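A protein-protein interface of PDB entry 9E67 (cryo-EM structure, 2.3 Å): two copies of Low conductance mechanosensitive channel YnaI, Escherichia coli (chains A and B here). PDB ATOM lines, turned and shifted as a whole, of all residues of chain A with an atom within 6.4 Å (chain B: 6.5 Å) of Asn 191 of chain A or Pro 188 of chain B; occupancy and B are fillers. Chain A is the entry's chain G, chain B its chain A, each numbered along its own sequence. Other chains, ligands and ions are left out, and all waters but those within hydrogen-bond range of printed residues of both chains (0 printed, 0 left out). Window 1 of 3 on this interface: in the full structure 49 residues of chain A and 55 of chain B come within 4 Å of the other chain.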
ATOM      1  N   SER A 187      -9.060  -1.649 -33.660  1.00  0.00           N
ATOM      2  CA  SER A 187      -7.980  -2.567 -33.994  1.00  0.00           C
ATOM      3  C   SER A 187      -8.489  -4.002 -33.986  1.00  0.00           C
ATOM      4  O   SER A 187      -9.158  -4.417 -33.033  1.00  0.00           O
ATOM      5  CB  SER A 187      -6.813  -2.415 -33.018  1.00  0.00           C
ATOM      6  OG  SER A 187      -5.768  -3.317 -33.332  1.00  0.00           O
ATOM      7  N   ASP A 189      -6.583  -6.532 -33.607  1.00  0.00           N
ATOM      8  CA  ASP A 189      -5.646  -7.299 -32.796  1.00  0.00           C
ATOM      9  C   ASP A 189      -5.859  -7.116 -31.299  1.00  0.00           C
ATOM     10  O   ASP A 189      -5.801  -8.093 -30.548  1.00  0.00           O
ATOM     11  CB  ASP A 189      -4.207  -6.918 -33.151  1.00  0.00           C
ATOM     12  CG  ASP A 189      -3.905  -7.091 -34.627  1.00  0.00           C
ATOM     13  OD1 ASP A 189      -3.905  -8.244 -35.104  1.00  0.00           O
ATOM     14  OD2 ASP A 189      -3.670  -6.075 -35.311  1.00  0.00           O
ATOM     15  N   ARG A 190      -6.099  -5.888 -30.846  1.00  0.00           N
ATOM     16  CA  ARG A 190      -6.324  -5.596 -29.438  1.00  0.00           C
ATOM     17  C   ARG A 190      -7.595  -4.773 -29.290  1.00  0.00           C
ATOM     18  O   ARG A 190      -8.151  -4.269 -30.267  1.00  0.00           O
ATOM     19  CB  ARG A 190      -5.141  -4.838 -28.816  1.00  0.00           C
ATOM     20  CG  ARG A 190      -3.779  -5.439 -29.104  1.00  0.00           C
ATOM     21  CD  ARG A 190      -3.387  -6.446 -28.041  1.00  0.00           C
ATOM     22  NE  ARG A 190      -3.144  -5.810 -26.752  1.00  0.00           N
ATOM     23  CZ  ARG A 190      -1.944  -5.626 -26.221  1.00  0.00           C
ATOM     24  NH1 ARG A 190      -0.845  -6.012 -26.846  1.00  0.00           N
ATOM     25  NH2 ARG A 190      -1.844  -5.039 -25.031  1.00  0.00           N
ATOM     26  N   ASN A 191      -8.049  -4.636 -28.046  1.00  0.00           N
ATOM     27  CA  ASN A 191      -9.228  -3.833 -27.731  1.00  0.00           C
ATOM     28  C   ASN A 191      -8.764  -2.432 -27.353  1.00  0.00           C
ATOM     29  O   ASN A 191      -8.322  -2.194 -26.228  1.00  0.00           O
ATOM     30  CB  ASN A 191     -10.036  -4.481 -26.613  1.00  0.00           C
ATOM     31  CG  ASN A 191     -11.400  -3.848 -26.433  1.00  0.00           C
ATOM     32  OD1 ASN A 191     -11.676  -2.772 -26.959  1.00  0.00           O
ATOM     33  ND2 ASN A 191     -12.264  -4.515 -25.682  1.00  0.00           N
ATOM     34  N   ILE A 192      -8.858  -1.501 -28.303  1.00  0.00           N
ATOM     35  CA  ILE A 192      -8.511  -0.105 -28.067  1.00  0.00           C
ATOM     36  C   ILE A 192      -9.638   0.788 -28.567  1.00  0.00           C
ATOM     37  O   ILE A 192      -9.427   1.970 -28.851  1.00  0.00           O
ATOM     38  CB  ILE A 192      -7.177   0.267 -28.744  1.00  0.00           C
ATOM     39  CG1 ILE A 192      -7.260   0.036 -30.253  1.00  0.00           C
ATOM     40  CG2 ILE A 192      -6.027  -0.521 -28.140  1.00  0.00           C
ATOM     41  CD1 ILE A 192      -6.220   0.789 -31.043  1.00  0.00           C
ATOM     42  N   GLU A 193     -10.843   0.230 -28.677  1.00  0.00           N
ATOM     43  CA  GLU A 193     -11.948   0.933 -29.315  1.00  0.00           C
ATOM     44  C   GLU A 193     -12.366   2.164 -28.517  1.00  0.00           C
ATOM     45  O   GLU A 193     -12.429   2.136 -27.286  1.00  0.00           O
ATOM     46  CB  GLU A 193     -13.138  -0.009 -29.484  1.00  0.00           C
ATOM     47  CG  GLU A 193     -14.313   0.599 -30.224  1.00  0.00           C
ATOM     48  CD  GLU A 193     -14.830  -0.290 -31.331  1.00  0.00           C
ATOM     49  OE1 GLU A 193     -14.686  -1.525 -31.223  1.00  0.00           O
ATOM     50  OE2 GLU A 193     -15.388   0.244 -32.311  1.00  0.00           O
ATOM     51  N   LEU A 214      -9.449   5.128 -21.171  1.00  0.00           N
ATOM     52  CA  LEU A 214      -8.608   3.965 -21.409  1.00  0.00           C
ATOM     53  C   LEU A 214      -7.220   4.453 -21.800  1.00  0.00           C
ATOM     54  O   LEU A 214      -7.087   5.326 -22.661  1.00  0.00           O
ATOM     55  CB  LEU A 214      -9.202   3.081 -22.509  1.00  0.00           C
ATOM     56  CG  LEU A 214      -8.392   1.881 -22.992  1.00  0.00           C
ATOM     57  CD1 LEU A 214      -8.492   0.731 -22.010  1.00  0.00           C
ATOM     58  CD2 LEU A 214      -8.859   1.449 -24.368  1.00  0.00           C
ATOM     59  N   VAL A 216      -3.782   3.522 -23.360  1.00  0.00           N
ATOM     60  CA  VAL A 216      -3.121   2.555 -24.234  1.00  0.00           C
ATOM     61  C   VAL A 216      -1.640   2.901 -24.293  1.00  0.00           C
ATOM     62  O   VAL A 216      -1.298   4.044 -24.627  1.00  0.00           O
ATOM     63  CB  VAL A 216      -3.742   2.559 -25.639  1.00  0.00           C
ATOM     64  CG1 VAL A 216      -3.103   1.492 -26.504  1.00  0.00           C
ATOM     65  CG2 VAL A 216      -5.241   2.349 -25.553  1.00  0.00           C
ATOM     66  N   ARG B 186      -9.546  -1.645 -14.643  1.00  0.00           N
ATOM     67  CA  ARG B 186      -9.860  -2.817 -15.445  1.00  0.00           C
ATOM     68  C   ARG B 186      -8.837  -2.934 -16.563  1.00  0.00           C
ATOM     69  O   ARG B 186      -8.036  -2.028 -16.798  1.00  0.00           O
ATOM     70  CB  ARG B 186     -11.276  -2.728 -16.017  1.00  0.00           C
ATOM     71  CG  ARG B 186     -12.100  -3.976 -15.848  1.00  0.00           C
ATOM     72  CD  ARG B 186     -13.448  -3.826 -16.524  1.00  0.00           C
ATOM     73  NE  ARG B 186     -13.308  -3.441 -17.922  1.00  0.00           N
ATOM     74  CZ  ARG B 186     -13.029  -4.282 -18.908  1.00  0.00           C
ATOM     75  NH1 ARG B 186     -12.857  -5.574 -18.684  1.00  0.00           N
ATOM     76  NH2 ARG B 186     -12.920  -3.816 -20.147  1.00  0.00           N
ATOM     77  N   SER B 187      -8.879  -4.063 -17.262  1.00  0.00           N
ATOM     78  CA  SER B 187      -8.019  -4.269 -18.419  1.00  0.00           C
ATOM     79  C   SER B 187      -8.632  -5.303 -19.354  1.00  0.00           C
ATOM     80  O   SER B 187      -9.054  -6.375 -18.906  1.00  0.00           O
ATOM     81  CB  SER B 187      -6.622  -4.710 -17.986  1.00  0.00           C
ATOM     82  OG  SER B 187      -5.784  -4.908 -19.108  1.00  0.00           O
ATOM     83  N   PRO B 188      -8.708  -5.017 -20.657  1.00  0.00           N
ATOM     84  CA  PRO B 188      -9.174  -6.033 -21.610  1.00  0.00           C
ATOM     85  C   PRO B 188      -8.152  -7.117 -21.914  1.00  0.00           C
ATOM     86  O   PRO B 188      -8.512  -8.113 -22.553  1.00  0.00           O
ATOM     87  CB  PRO B 188      -9.488  -5.210 -22.865  1.00  0.00           C
ATOM     88  CG  PRO B 188      -8.619  -4.008 -22.750  1.00  0.00           C
ATOM     89  CD  PRO B 188      -8.533  -3.700 -21.288  1.00  0.00           C
ATOM     90  N   ASP B 189      -6.903  -6.963 -21.479  1.00  0.00           N
ATOM     91  CA  ASP B 189      -5.850  -7.932 -21.757  1.00  0.00           C
ATOM     92  C   ASP B 189      -5.640  -8.931 -20.626  1.00  0.00           C
ATOM     93  O   ASP B 189      -5.454 -10.122 -20.888  1.00  0.00           O
ATOM     94  CB  ASP B 189      -4.530  -7.211 -22.046  1.00  0.00           C
ATOM     95  CG  ASP B 189      -4.655  -6.183 -23.151  1.00  0.00           C
ATOM     96  OD1 ASP B 189      -5.067  -6.555 -24.268  1.00  0.00           O
ATOM     97  OD2 ASP B 189      -4.340  -5.001 -22.904  1.00  0.00           O
ATOM     98  N   ARG B 190      -5.660  -8.475 -19.376  1.00  0.00           N
ATOM     99  CA  ARG B 190      -5.469  -9.337 -18.220  1.00  0.00           C
ATOM    100  C   ARG B 190      -6.570  -9.071 -17.204  1.00  0.00           C
ATOM    101  O   ARG B 190      -7.297  -8.079 -17.289  1.00  0.00           O
ATOM    102  CB  ARG B 190      -4.097  -9.118 -17.564  1.00  0.00           C
ATOM    103  CG  ARG B 190      -2.923  -9.144 -18.524  1.00  0.00           C
ATOM    104  CD  ARG B 190      -2.356 -10.543 -18.658  1.00  0.00           C
ATOM    105  NE  ARG B 190      -1.728 -10.997 -17.423  1.00  0.00           N
ATOM    106  CZ  ARG B 190      -0.420 -11.104 -17.241  1.00  0.00           C
ATOM    107  NH1 ARG B 190       0.438 -10.797 -18.199  1.00  0.00           N
ATOM    108  NH2 ARG B 190       0.039 -11.535 -16.071  1.00  0.00           N
ATOM    109  N   SER B 225      -3.273  -2.267 -21.751  1.00  0.00           N
ATOM    110  CA  SER B 225      -4.183  -1.132 -21.701  1.00  0.00           C
ATOM    111  C   SER B 225      -4.981  -1.175 -20.407  1.00  0.00           C
ATOM    112  O   SER B 225      -5.558  -2.205 -20.057  1.00  0.00           O
ATOM    113  CB  SER B 225      -5.124  -1.144 -22.904  1.00  0.00           C
ATOM    114  OG  SER B 225      -4.403  -1.111 -24.121  1.00  0.00           O
ATOM    115  N   VAL B 226      -5.014  -0.050 -19.699  1.00  0.00           N
ATOM    116  CA  VAL B 226      -5.672   0.051 -18.403  1.00  0.00           C
ATOM    117  C   VAL B 226      -6.897   0.940 -18.558  1.00  0.00           C
ATOM    118  O   VAL B 226      -6.786   2.093 -18.989  1.00  0.00           O
ATOM    119  CB  VAL B 226      -4.725   0.600 -17.327  1.00  0.00           C
ATOM    120  CG1 VAL B 226      -5.477   0.845 -16.033  1.00  0.00           C
ATOM    121  CG2 VAL B 226      -3.574  -0.359 -17.099  1.00  0.00           C
ATOM    122  N   GLU B 227      -8.059   0.403 -18.209  1.00  0.00           N
ATOM    123  CA  GLU B 227      -9.299   1.161 -18.174  1.00  0.00           C
ATOM    124  C   GLU B 227      -9.593   1.590 -16.743  1.00  0.00           C
ATOM    125  O   GLU B 227      -9.263   0.888 -15.786  1.00  0.00           O
ATOM    126  CB  GLU B 227     -10.460   0.331 -18.725  1.00  0.00           C
ATOM    127  CG  GLU B 227     -11.597   1.149 -19.299  1.00  0.00           C
ATOM    128  CD  GLU B 227     -12.902   0.381 -19.335  1.00  0.00           C
ATOM    129  OE1 GLU B 227     -13.363  -0.059 -18.263  1.00  0.00           O
ATOM    130  OE2 GLU B 227     -13.467   0.213 -20.435  1.00  0.00           O
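NE of Arg 186 of chain B lies within salt-bridge range of OE1 of Glu 227 of chain B, at 3.4 Å. OG of Ser 187 of chain B lies close to N of Asp 189 of chain B (3.3 Å). OG of Ser 187 of chain B lies within hydrogen-bond range of O of Ser 225 of chain B (2.9 Å). OD2 of Asp 189 of chain B lies within hydrogen-bond range of N of Ser 225 of chain B, 3.2 Å away.
Arg 190 of chain A touches Asp 189 of chain B, but with the chains exchanged Asp 189 of chain A does not touch Arg 190 of chain B (11.2 Å).
Among the printed residues, pairs that only touch across the chains: Asn 191 of chain A with Pro 188 of chain B, Leu 214 of chain A with Ser 225 of chain B, Leu 214 of chain A with Val 226 of chain B, Leu 214 of chain A with Glu 227 of chain B and Val 216 of chain A with Ser 225 of chain B.
The guanidinium group of Arg 190 of chain A lies within salt-bridge range of the side-chain carboxylate of Asp 189 of chain B (3.2 Å).
Of chain B, only Pro 188 (3.9 Å) comes within 4 Å of Asn 191 of chain A. Of chain A, only Asn 191 comes within 4 Å of Pro 188 of chain B. Printed residues of chain B within 4 Å of Arg 190 of chain A: Asp 189 (3.2 Å). Printed residues of chain A within 4 Å of Asp 189 of chain B: Arg 190 (3.2 Å). Of the printed residues of chain B, Val 216 of chain A touches Ser 225 (3.8 Å). Printed residues of chain A within 4 Å of Val 226 of chain B: Leu 214. Of the printed residues of chain A, Glu 227 of chain B touches Leu 214. Ser 187 of chain B touches none of the printed residues of chain A. Arg 186 of chain B touches none of the printed residues of chain A. The nearest residue of chain B that does not touch Asn 191 of chain A is Ser 225 of chain B (4.6 Å). The nearest residue of chain A that does not touch Pro 188 of chain B is Leu 214 of chain A (4.5 Å).
Of the 8 printed residues of chain A, 4 touch a printed residue of chain B. Hydrophobic or aromatic side chains of chain A that line the printed part of chain B: Leu 214 and Val 216. Of the 8 printed residues of chain B, 5 touch a printed residue of chain A. Hydrophobic or aromatic side chains of chain B that line the printed part of chain A: Pro 188.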
